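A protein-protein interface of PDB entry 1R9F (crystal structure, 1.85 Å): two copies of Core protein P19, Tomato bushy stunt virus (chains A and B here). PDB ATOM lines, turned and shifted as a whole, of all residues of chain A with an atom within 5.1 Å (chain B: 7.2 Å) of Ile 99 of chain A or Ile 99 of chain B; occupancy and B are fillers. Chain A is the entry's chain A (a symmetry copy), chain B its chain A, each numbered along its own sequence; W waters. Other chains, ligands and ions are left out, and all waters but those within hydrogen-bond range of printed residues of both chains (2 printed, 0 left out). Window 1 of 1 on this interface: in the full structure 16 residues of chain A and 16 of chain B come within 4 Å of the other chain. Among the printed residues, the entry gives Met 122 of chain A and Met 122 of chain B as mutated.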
ATOM      1  N   TYR A  90      12.317  30.205 -19.966  1.00  0.00           N
ATOM      2  CA  TYR A  90      11.616  30.194 -21.238  1.00  0.00           C
ATOM      3  C   TYR A  90      10.636  29.039 -21.127  1.00  0.00           C
ATOM      4  O   TYR A  90      11.014  27.948 -20.698  1.00  0.00           O
ATOM      5  CB  TYR A  90      12.553  29.920 -22.416  1.00  0.00           C
ATOM      6  CG  TYR A  90      11.786  29.670 -23.703  1.00  0.00           C
ATOM      7  CD1 TYR A  90      11.143  30.716 -24.369  1.00  0.00           C
ATOM      8  CD2 TYR A  90      11.646  28.380 -24.217  1.00  0.00           C
ATOM      9  CE1 TYR A  90      10.376  30.487 -25.513  1.00  0.00           C
ATOM     10  CE2 TYR A  90      10.877  28.138 -25.364  1.00  0.00           C
ATOM     11  CZ  TYR A  90      10.245  29.194 -26.004  1.00  0.00           C
ATOM     12  OH  TYR A  90       9.472  28.965 -27.121  1.00  0.00           O
ATOM     13  N   SER A  91       9.383  29.274 -21.501  1.00  0.00           N
ATOM     14  CA  SER A  91       8.374  28.226 -21.456  1.00  0.00           C
ATOM     15  C   SER A  91       7.615  28.171 -22.768  1.00  0.00           C
ATOM     16  O   SER A  91       7.393  29.196 -23.412  1.00  0.00           O
ATOM     17  CB  SER A  91       7.370  28.476 -20.327  1.00  0.00           C
ATOM     18  OG  SER A  91       7.986  28.392 -19.058  1.00  0.00           O
ATOM     19  N   ILE A  92       7.227  26.971 -23.170  1.00  0.00           N
ATOM     20  CA  ILE A  92       6.448  26.814 -24.386  1.00  0.00           C
ATOM     21  C   ILE A  92       5.466  25.679 -24.156  1.00  0.00           C
ATOM     22  O   ILE A  92       5.833  24.616 -23.651  1.00  0.00           O
ATOM     23  CB  ILE A  92       7.331  26.499 -25.624  1.00  0.00           C
ATOM     24  CG1 ILE A  92       6.439  26.325 -26.861  1.00  0.00           C
ATOM     25  CG2 ILE A  92       8.164  25.244 -25.389  1.00  0.00           C
ATOM     26  CD1 ILE A  92       7.207  26.242 -28.179  1.00  0.00           C
ATOM     27  N   VAL A  97       1.424  19.589 -23.832  1.00  0.00           N
ATOM     28  CA  VAL A  97       2.755  19.406 -23.263  1.00  0.00           C
ATOM     29  C   VAL A  97       3.455  20.744 -23.086  1.00  0.00           C
ATOM     30  O   VAL A  97       3.329  21.642 -23.920  1.00  0.00           O
ATOM     31  CB  VAL A  97       3.637  18.498 -24.147  1.00  0.00           C
ATOM     32  CG1 VAL A  97       4.999  18.301 -23.493  1.00  0.00           C
ATOM     33  CG2 VAL A  97       2.955  17.153 -24.350  1.00  0.00           C
ATOM     34  N   SER A  98       4.195  20.864 -21.994  1.00  0.00           N
ATOM     35  CA  SER A  98       4.915  22.086 -21.687  1.00  0.00           C
ATOM     36  C   SER A  98       6.385  21.806 -21.419  1.00  0.00           C
ATOM     37  O   SER A  98       6.727  20.824 -20.764  1.00  0.00           O
ATOM     38  CB  SER A  98       4.295  22.750 -20.457  1.00  0.00           C
ATOM     39  OG  SER A  98       5.176  23.705 -19.899  1.00  0.00           O
ATOM     40  N   ILE A  99       7.252  22.663 -21.940  1.00  0.00           N
ATOM     41  CA  ILE A  99       8.680  22.527 -21.717  1.00  0.00           C
ATOM     42  C   ILE A  99       9.145  23.863 -21.180  1.00  0.00           C
ATOM     43  O   ILE A  99       8.786  24.915 -21.713  1.00  0.00           O
ATOM     44  CB  ILE A  99       9.460  22.214 -23.010  1.00  0.00           C
ATOM     45  CG1 ILE A  99       9.096  20.818 -23.522  1.00  0.00           C
ATOM     46  CG2 ILE A  99      10.964  22.294 -22.739  1.00  0.00           C
ATOM     47  CD1 ILE A  99       9.879  20.392 -24.762  1.00  0.00           C
ATOM     48  N   THR A 100       9.923  23.822 -20.108  1.00  0.00           N
ATOM     49  CA  THR A 100      10.439  25.035 -19.497  1.00  0.00           C
ATOM     50  C   THR A 100      11.939  24.893 -19.331  1.00  0.00           C
ATOM     51  O   THR A 100      12.421  23.889 -18.810  1.00  0.00           O
ATOM     52  CB  THR A 100       9.799  25.269 -18.118  1.00  0.00           C
ATOM     53  OG1 THR A 100       8.389  25.471 -18.279  1.00  0.00           O
ATOM     54  CG2 THR A 100      10.401  26.485 -17.440  1.00  0.00           C
ATOM     55  N   VAL A 101      12.675  25.897 -19.791  1.00  0.00           N
ATOM     56  CA  VAL A 101      14.122  25.902 -19.681  1.00  0.00           C
ATOM     57  C   VAL A 101      14.423  27.019 -18.689  1.00  0.00           C
ATOM     58  O   VAL A 101      14.042  28.164 -18.915  1.00  0.00           O
ATOM     59  CB  VAL A 101      14.778  26.225 -21.038  1.00  0.00           C
ATOM     60  CG1 VAL A 101      16.290  26.141 -20.922  1.00  0.00           C
ATOM     61  CG2 VAL A 101      14.268  25.257 -22.102  1.00  0.00           C
ATOM     62  N   SER A 102      15.088  26.693 -17.585  1.00  0.00           N
ATOM     63  CA  SER A 102      15.380  27.705 -16.573  1.00  0.00           C
ATOM     64  C   SER A 102      16.820  27.670 -16.087  1.00  0.00           C
ATOM     65  O   SER A 102      17.509  26.653 -16.205  1.00  0.00           O
ATOM     66  CB  SER A 102      14.441  27.539 -15.369  1.00  0.00           C
ATOM     67  OG  SER A 102      14.472  26.223 -14.864  1.00  0.00           O
ATOM     68  N   MET A 114      19.317  25.937 -25.537  1.00  0.00           N
ATOM     69  CA  MET A 114      18.415  24.854 -25.164  1.00  0.00           C
ATOM     70  C   MET A 114      16.976  25.239 -25.472  1.00  0.00           C
ATOM     71  O   MET A 114      16.175  24.402 -25.898  1.00  0.00           O
ATOM     72  CB  MET A 114      18.541  24.538 -23.672  1.00  0.00           C
ATOM     73  CG  MET A 114      19.844  23.866 -23.286  1.00  0.00           C
ATOM     74  SD  MET A 114      20.081  22.207 -24.244  1.00  0.00           S
ATOM     75  CE  MET A 114      21.445  22.784 -25.492  1.00  0.00           C
ATOM     76  N   SER A 118      14.408  23.211 -27.898  1.00  0.00           N
ATOM     77  CA  SER A 118      13.185  22.661 -27.323  1.00  0.00           C
ATOM     78  C   SER A 118      11.980  23.154 -28.123  1.00  0.00           C
ATOM     79  O   SER A 118      11.021  22.417 -28.354  1.00  0.00           O
ATOM     80  CB  SER A 118      13.033  23.102 -25.864  1.00  0.00           C
ATOM     81  OG  SER A 118      14.160  22.731 -25.093  1.00  0.00           O
ATOM     82  N   MET A 122       9.436  20.770 -30.017  1.00  0.00           N
ATOM     83  CA  MET A 122       8.052  20.843 -29.573  1.00  0.00           C
ATOM     84  C   MET A 122       7.098  21.032 -30.752  1.00  0.00           C
ATOM     85  O   MET A 122       6.073  20.357 -30.860  1.00  0.00           O
ATOM     86  CB  MET A 122       7.884  22.007 -28.590  1.00  0.00           C
ATOM     87  CG  MET A 122       6.504  22.097 -27.969  1.00  0.00           C
ATOM     88  SD  MET A 122       6.261  20.804 -26.547  1.00  0.00           S
ATOM     89  CE  MET A 122       6.110  22.040 -25.076  1.00  0.00           C
ATOM     90  N   LYS B  38      21.429  15.586 -12.625  1.00  0.00           N
ATOM     91  CA  LYS B  38      20.287  15.172 -11.822  1.00  0.00           C
ATOM     92  C   LYS B  38      19.045  15.166 -12.694  1.00  0.00           C
ATOM     93  O   LYS B  38      18.826  16.089 -13.479  1.00  0.00           O
ATOM     94  CB  LYS B  38      20.073  16.144 -10.662  1.00  0.00           C
ATOM     95  CG  LYS B  38      21.186  16.149  -9.633  1.00  0.00           C
ATOM     96  CD  LYS B  38      21.163  17.411  -8.775  1.00  0.00           C
ATOM     97  CE  LYS B  38      19.819  17.620  -8.096  1.00  0.00           C
ATOM     98  NZ  LYS B  38      19.793  18.897  -7.322  1.00  0.00           N
ATOM     99  N   THR B  89       5.705  15.071 -14.576  1.00  0.00           N
ATOM    100  CA  THR B  89       6.823  15.939 -14.897  1.00  0.00           C
ATOM    101  C   THR B  89       8.179  15.244 -14.915  1.00  0.00           C
ATOM    102  O   THR B  89       8.473  14.386 -14.077  1.00  0.00           O
ATOM    103  CB  THR B  89       6.919  17.106 -13.893  1.00  0.00           C
ATOM    104  OG1 THR B  89       7.879  18.059 -14.360  1.00  0.00           O
ATOM    105  CG2 THR B  89       7.354  16.597 -12.533  1.00  0.00           C
ATOM    106  N   TYR B  90       8.997  15.619 -15.893  1.00  0.00           N
ATOM    107  CA  TYR B  90      10.350  15.099 -15.994  1.00  0.00           C
ATOM    108  C   TYR B  90      11.242  16.326 -15.919  1.00  0.00           C
ATOM    109  O   TYR B  90      10.982  17.320 -16.598  1.00  0.00           O
ATOM    110  CB  TYR B  90      10.605  14.399 -17.331  1.00  0.00           C
ATOM    111  CG  TYR B  90      12.076  14.075 -17.528  1.00  0.00           C
ATOM    112  CD1 TYR B  90      12.688  13.052 -16.799  1.00  0.00           C
ATOM    113  CD2 TYR B  90      12.869  14.831 -18.392  1.00  0.00           C
ATOM    114  CE1 TYR B  90      14.055  12.793 -16.919  1.00  0.00           C
ATOM    115  CE2 TYR B  90      14.242  14.579 -18.520  1.00  0.00           C
ATOM    116  CZ  TYR B  90      14.826  13.562 -17.780  1.00  0.00           C
ATOM    117  OH  TYR B  90      16.178  13.318 -17.884  1.00  0.00           O
ATOM    118  N   SER B  91      12.280  16.266 -15.091  1.00  0.00           N
ATOM    119  CA  SER B  91      13.208  17.381 -14.966  1.00  0.00           C
ATOM    120  C   SER B  91      14.638  16.887 -15.070  1.00  0.00           C
ATOM    121  O   SER B  91      14.958  15.782 -14.633  1.00  0.00           O
ATOM    122  CB  SER B  91      13.038  18.089 -13.619  1.00  0.00           C
ATOM    123  OG  SER B  91      11.770  18.705 -13.513  1.00  0.00           O
ATOM    124  N   ILE B  92      15.497  17.702 -15.661  1.00  0.00           N
ATOM    125  CA  ILE B  92      16.902  17.349 -15.765  1.00  0.00           C
ATOM    126  C   ILE B  92      17.707  18.627 -15.623  1.00  0.00           C
ATOM    127  O   ILE B  92      17.396  19.645 -16.246  1.00  0.00           O
ATOM    128  CB  ILE B  92      17.246  16.661 -17.116  1.00  0.00           C
ATOM    129  CG1 ILE B  92      18.746  16.339 -17.161  1.00  0.00           C
ATOM    130  CG2 ILE B  92      16.858  17.553 -18.290  1.00  0.00           C
ATOM    131  CD1 ILE B  92      19.160  15.457 -18.337  1.00  0.00           C
ATOM    132  N   ARG B  93      18.718  18.579 -14.765  1.00  0.00           N
ATOM    133  CA  ARG B  93      19.583  19.725 -14.556  1.00  0.00           C
ATOM    134  C   ARG B  93      21.020  19.326 -14.848  1.00  0.00           C
ATOM    135  O   ARG B  93      21.492  18.286 -14.384  1.00  0.00           O
ATOM    136  CB  ARG B  93      19.474  20.241 -13.126  1.00  0.00           C
ATOM    137  CG  ARG B  93      20.527  21.292 -12.819  1.00  0.00           C
ATOM    138  CD  ARG B  93      20.154  22.166 -11.646  1.00  0.00           C
ATOM    139  NE  ARG B  93      21.118  23.255 -11.495  1.00  0.00           N
ATOM    140  CZ  ARG B  93      20.914  24.339 -10.755  1.00  0.00           C
ATOM    141  NH1 ARG B  93      21.850  25.276 -10.677  1.00  0.00           N
ATOM    142  NH2 ARG B  93      19.768  24.492 -10.102  1.00  0.00           N
ATOM    143  N   PHE B  94      21.706  20.154 -15.627  1.00  0.00           N
ATOM    144  CA  PHE B  94      23.087  19.885 -15.985  1.00  0.00           C
ATOM    145  C   PHE B  94      23.794  21.187 -16.331  1.00  0.00           C
ATOM    146  O   PHE B  94      23.345  21.934 -17.201  1.00  0.00           O
ATOM    147  CB  PHE B  94      23.135  18.936 -17.186  1.00  0.00           C
ATOM    148  CG  PHE B  94      24.523  18.511 -17.578  1.00  0.00           C
ATOM    149  CD1 PHE B  94      25.378  17.929 -16.646  1.00  0.00           C
ATOM    150  CD2 PHE B  94      24.958  18.650 -18.891  1.00  0.00           C
ATOM    151  CE1 PHE B  94      26.644  17.488 -17.018  1.00  0.00           C
ATOM    152  CE2 PHE B  94      26.222  18.212 -19.274  1.00  0.00           C
ATOM    153  CZ  PHE B  94      27.066  17.630 -18.338  1.00  0.00           C
ATOM    154  N   VAL B  97      21.830  24.651 -16.118  1.00  0.00           N
ATOM    155  CA  VAL B  97      20.591  24.760 -16.880  1.00  0.00           C
ATOM    156  C   VAL B  97      19.641  23.627 -16.529  1.00  0.00           C
ATOM    157  O   VAL B  97      20.060  22.488 -16.316  1.00  0.00           O
ATOM    158  CB  VAL B  97      20.850  24.736 -18.403  1.00  0.00           C
ATOM    159  CG1 VAL B  97      19.535  24.895 -19.156  1.00  0.00           C
ATOM    160  CG2 VAL B  97      21.808  25.856 -18.783  1.00  0.00           C
ATOM    161  N   SER B  98      18.357  23.950 -16.475  1.00  0.00           N
ATOM    162  CA  SER B  98      17.334  22.974 -16.144  1.00  0.00           C
ATOM    163  C   SER B  98      16.235  22.953 -17.194  1.00  0.00           C
ATOM    164  O   SER B  98      15.815  23.998 -17.684  1.00  0.00           O
ATOM    165  CB  SER B  98      16.726  23.314 -14.782  1.00  0.00           C
ATOM    166  OG  SER B  98      15.493  22.646 -14.598  1.00  0.00           O
ATOM    167  N   ILE B  99      15.782  21.757 -17.545  1.00  0.00           N
ATOM    168  CA  ILE B  99      14.704  21.608 -18.506  1.00  0.00           C
ATOM    169  C   ILE B  99      13.663  20.741 -17.829  1.00  0.00           C
ATOM    170  O   ILE B  99      13.992  19.715 -17.232  1.00  0.00           O
ATOM    171  CB  ILE B  99      15.154  20.916 -19.808  1.00  0.00           C
ATOM    172  CG1 ILE B  99      16.125  21.817 -20.577  1.00  0.00           C
ATOM    173  CG2 ILE B  99      13.933  20.605 -20.677  1.00  0.00           C
ATOM    174  CD1 ILE B  99      16.567  21.242 -21.921  1.00  0.00           C
ATOM    175  N   THR B 100      12.411  21.170 -17.901  1.00  0.00           N
ATOM    176  CA  THR B 100      11.319  20.428 -17.297  1.00  0.00           C
ATOM    177  C   THR B 100      10.232  20.232 -18.335  1.00  0.00           C
ATOM    178  O   THR B 100       9.817  21.182 -18.996  1.00  0.00           O
ATOM    179  CB  THR B 100      10.736  21.193 -16.095  1.00  0.00           C
ATOM    180  OG1 THR B 100      11.742  21.320 -15.082  1.00  0.00           O
ATOM    181  CG2 THR B 100       9.538  20.463 -15.518  1.00  0.00           C
ATOM    182  N   VAL B 101       9.786  18.991 -18.486  1.00  0.00           N
ATOM    183  CA  VAL B 101       8.736  18.663 -19.433  1.00  0.00           C
ATOM    184  C   VAL B 101       7.550  18.268 -18.559  1.00  0.00           C
ATOM    185  O   VAL B 101       7.657  17.347 -17.754  1.00  0.00           O
ATOM    186  CB  VAL B 101       9.144  17.470 -20.319  1.00  0.00           C
ATOM    187  CG1 VAL B 101       8.068  17.198 -21.357  1.00  0.00           C
ATOM    188  CG2 VAL B 101      10.479  17.764 -20.997  1.00  0.00           C
ATOM    189  N   SER B 102       6.428  18.967 -18.699  1.00  0.00           N
ATOM    190  CA  SER B 102       5.263  18.668 -17.870  1.00  0.00           C
ATOM    191  C   SER B 102       3.969  18.584 -18.661  1.00  0.00           C
ATOM    192  O   SER B 102       3.858  19.129 -19.763  1.00  0.00           O
ATOM    193  CB  SER B 102       5.110  19.726 -16.768  1.00  0.00           C
ATOM    194  OG  SER B 102       5.092  21.032 -17.301  1.00  0.00           O
ATOM    195  N   LEU B 111       4.900  13.254 -23.604  1.00  0.00           N
ATOM    196  CA  LEU B 111       5.771  13.799 -22.568  1.00  0.00           C
ATOM    197  C   LEU B 111       7.109  13.056 -22.581  1.00  0.00           C
ATOM    198  O   LEU B 111       8.172  13.675 -22.529  1.00  0.00           O
ATOM    199  CB  LEU B 111       5.112  13.651 -21.195  1.00  0.00           C
ATOM    200  CG  LEU B 111       3.968  14.592 -20.818  1.00  0.00           C
ATOM    201  CD1 LEU B 111       3.573  14.332 -19.368  1.00  0.00           C
ATOM    202  CD2 LEU B 111       4.406  16.035 -20.989  1.00  0.00           C
ATOM    203  N   MET B 114       9.269  13.950 -25.660  1.00  0.00           N
ATOM    204  CA  MET B 114       9.908  15.248 -25.478  1.00  0.00           C
ATOM    205  C   MET B 114      10.986  15.158 -24.408  1.00  0.00           C
ATOM    206  O   MET B 114      12.042  15.785 -24.521  1.00  0.00           O
ATOM    207  CB  MET B 114       8.879  16.302 -25.064  1.00  0.00           C
ATOM    208  CG  MET B 114       7.914  16.696 -26.166  1.00  0.00           C
ATOM    209  SD  MET B 114       8.858  17.391 -27.699  1.00  0.00           S
ATOM    210  CE  MET B 114       8.647  15.872 -28.883  1.00  0.00           C
ATOM    211  N   ALA B 115      10.720  14.371 -23.368  1.00  0.00           N
ATOM    212  CA  ALA B 115      11.676  14.220 -22.280  1.00  0.00           C
ATOM    213  C   ALA B 115      12.991  13.600 -22.737  1.00  0.00           C
ATOM    214  O   ALA B 115      14.070  14.105 -22.424  1.00  0.00           O
ATOM    215  CB  ALA B 115      11.065  13.377 -21.152  1.00  0.00           C
ATOM    216  N   ARG B 117      14.214  13.509 -25.711  1.00  0.00           N
ATOM    217  CA  ARG B 117      14.897  14.393 -26.651  1.00  0.00           C
ATOM    218  C   ARG B 117      15.590  15.526 -25.905  1.00  0.00           C
ATOM    219  O   ARG B 117      16.714  15.899 -26.240  1.00  0.00           O
ATOM    220  CB  ARG B 117      13.909  14.952 -27.676  1.00  0.00           C
ATOM    221  CG  ARG B 117      13.436  13.904 -28.666  1.00  0.00           C
ATOM    222  CD  ARG B 117      12.354  14.426 -29.588  1.00  0.00           C
ATOM    223  NE  ARG B 117      11.935  13.407 -30.547  1.00  0.00           N
ATOM    224  CZ  ARG B 117      10.926  13.549 -31.401  1.00  0.00           C
ATOM    225  NH1 ARG B 117      10.222  14.676 -31.420  1.00  0.00           N
ATOM    226  NH2 ARG B 117      10.619  12.567 -32.238  1.00  0.00           N
ATOM    227  N   SER B 118      14.928  16.062 -24.883  1.00  0.00           N
ATOM    228  CA  SER B 118      15.502  17.143 -24.087  1.00  0.00           C
ATOM    229  C   SER B 118      16.734  16.628 -23.343  1.00  0.00           C
ATOM    230  O   SER B 118      17.736  17.330 -23.202  1.00  0.00           O
ATOM    231  CB  SER B 118      14.481  17.660 -23.071  1.00  0.00           C
ATOM    232  OG  SER B 118      13.289  18.084 -23.706  1.00  0.00           O
ATOM    233  N   LYS B 119      16.647  15.395 -22.858  1.00  0.00           N
ATOM    234  CA  LYS B 119      17.755  14.788 -22.131  1.00  0.00           C
ATOM    235  C   LYS B 119      18.980  14.678 -23.035  1.00  0.00           C
ATOM    236  O   LYS B 119      20.086  15.076 -22.658  1.00  0.00           O
ATOM    237  CB  LYS B 119      17.344  13.402 -21.621  1.00  0.00           C
ATOM    238  CG  LYS B 119      18.405  12.697 -20.787  1.00  0.00           C
ATOM    239  CD  LYS B 119      17.845  11.418 -20.176  1.00  0.00           C
ATOM    240  CE  LYS B 119      18.897  10.703 -19.352  1.00  0.00           C
ATOM    241  NZ  LYS B 119      18.339   9.522 -18.650  1.00  0.00           N
ATOM    242  N   GLU B 121      19.664  16.330 -25.800  1.00  0.00           N
ATOM    243  CA  GLU B 121      20.181  17.647 -26.160  1.00  0.00           C
ATOM    244  C   GLU B 121      20.919  18.287 -24.996  1.00  0.00           C
ATOM    245  O   GLU B 121      21.948  18.930 -25.179  1.00  0.00           O
ATOM    246  CB  GLU B 121      19.042  18.563 -26.612  1.00  0.00           C
ATOM    247  CG  GLU B 121      18.535  18.274 -28.016  1.00  0.00           C
ATOM    248  CD  GLU B 121      19.612  18.460 -29.075  1.00  0.00           C
ATOM    249  OE1 GLU B 121      20.200  19.562 -29.147  1.00  0.00           O
ATOM    250  OE2 GLU B 121      19.869  17.503 -29.837  1.00  0.00           O
ATOM    251  N   MET B 122      20.389  18.104 -23.793  1.00  0.00           N
ATOM    252  CA  MET B 122      20.994  18.668 -22.596  1.00  0.00           C
ATOM    253  C   MET B 122      22.400  18.109 -22.367  1.00  0.00           C
ATOM    254  O   MET B 122      23.345  18.850 -22.090  1.00  0.00           O
ATOM    255  CB  MET B 122      20.119  18.356 -21.376  1.00  0.00           C
ATOM    256  CG  MET B 122      20.595  19.003 -20.091  1.00  0.00           C
ATOM    257  SD  MET B 122      20.123  20.880 -20.006  1.00  0.00           S
ATOM    258  CE  MET B 122      18.880  20.784 -18.535  1.00  0.00           C
HETATM  259  O   HOH W   1      13.061  24.253 -16.166  1.00  0.00           O
HETATM  260  O   HOH W   2       7.465  22.215 -18.029  1.00  0.00           O
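Of the printed residues of chain B, Ile 99 of chain A touches Ile 99 (3.99 Å) and Thr 100 (3.2 Å). Printed residues of chain B within 4 Å of Thr 100 of chain A: Ser 98, Ile 99 and Thr 100. Printed residues of chain B within 4 Å of Ser 102 of chain A: Val 97 (3.7 Å) and Ser 98 (2.8 Å). Of the printed residues of chain A, Leu 111 of chain B touches Val 97 (3.4 Å). Printed residues of chain A within 4 Å of Glu 121 of chain B: Met 114. Printed residues of chain A within 4 Å of Val 97 of chain B: Val 101 and Ser 102. Arg 93 of chain B touches none of the printed residues of chain A. The nearest printed residue of chain A that does not touch Ile 99 of chain B is Val 101 of chain A (4.2 Å). The nearest printed residue of chain A that does not touch Ser 98 of chain B is Met 114 of chain A (6.6 Å).
Val 97 of chain A touches Ser 102 of chain B, and with the chains exchanged Ser 102 of chain A touches Val 97 of chain B. Ser 98 of chain A touches Thr 100 of chain B, and with the chains exchanged Thr 100 of chain A touches Ser 98 of chain B. Ile 99 of chain A touches Thr 100 of chain B, and with the chains exchanged Thr 100 of chain A touches Ile 99 of chain B. Thr 100 of chain B touches its own counterpart, Thr 100 of chain A. 12 positions are printed for both chains. Of the 16 pairs that touch across the chains among the printed residues, 14 have their exchanged pair printed and touching as well.
Among the printed residues, pairs that only touch across the chains: Val 97 of chain A with Val 101 of chain B, Val 97 of chain A with Ser 102 of chain B, Val 97 of chain A with Leu 111 of chain B, Ser 98 of chain A with Thr 100 of chain B, Ser 98 of chain A with Val 101 of chain B, Ile 99 of chain A with Ile 99 of chain B, Ile 99 of chain A with Thr 100 of chain B, Thr 100 of chain A with Ser 98 of chain B, Thr 100 of chain A with Ile 99 of chain B, Val 101 of chain A with Val 97 of chain B, Val 101 of chain A with Ser 98 of chain B, Ser 102 of chain A with Val 97 of chain B and Met 114 of chain A with Glu 121 of chain B.
The backbone carbonyl oxygen of Ser 98 of chain A is in hydrogen-bond range of the backbone NH of Ser 102 of chain B. N of Thr 100 of chain B sits at hydrogen-bond distance from O of Thr 100 of chain A (2.9 Å). The backbone carbonyl oxygen (O) of Ser 98 of chain B is in hydrogen-bond range of the backbone NH (N) of Ser 102 of chain A, at 2.8 Å.
The side-chain hydroxyl (OG) of Ser 91 of chain B is in hydrogen-bond range of the side-chain hydroxyl (OG1) of Thr 100 of chain B (3.0 Å). The backbone NH (N) of Val 101 of chain B sits at hydrogen-bond distance from the backbone carbonyl oxygen (O) of Tyr 90 of chain B, 2.8 Å away. The backbone carbonyl oxygen of Met 114 of chain A is in hydrogen-bond range of the side-chain hydroxyl of Ser 118 of chain A (2.7 Å). The backbone carbonyl oxygen (O) of Val 101 of chain B lies close to the side-chain hydroxyl (OG1) of Thr 89 of chain B (3.5 Å). The backbone NH of Ile 99 of chain A sits at hydrogen-bond distance from the backbone carbonyl oxygen of Ile 92 of chain A, 3.0 Å away. O of Tyr 90 of chain A lies within hydrogen-bond range of N of Val 101 of chain A (2.8 Å).
Printed residues of chain A that touch a printed residue of chain B: Val 97, Ser 98, Ile 99, Thr 100, Val 101, Ser 102 and Met 114. Hydrophobic or aromatic side chains of chain A that line the printed part of chain B: Val 97, Ile 99, Val 101 and Met 114. Among the printed residues, no Asp or Glu carboxylate lies within 4 Å of a Lys or Arg side-chain nitrogen of the other chain.
Water W1 lies within hydrogen-bond range of O of Thr 100 of chain A (2.7 Å), OG of Ser 102 of chain A (2.8 Å), O of Ser 98 of chain B (3.2 Å) and OG1 of Thr 100 of chain B (3.4 Å). Water W2 lies within hydrogen-bond range of O of Thr 100 of chain B (2.7 Å), OG of Ser 102 of chain B (2.7 Å), O of Ser 98 of chain A (3.2 Å) and OG1 of Thr 100 of chain A (3.4 Å).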
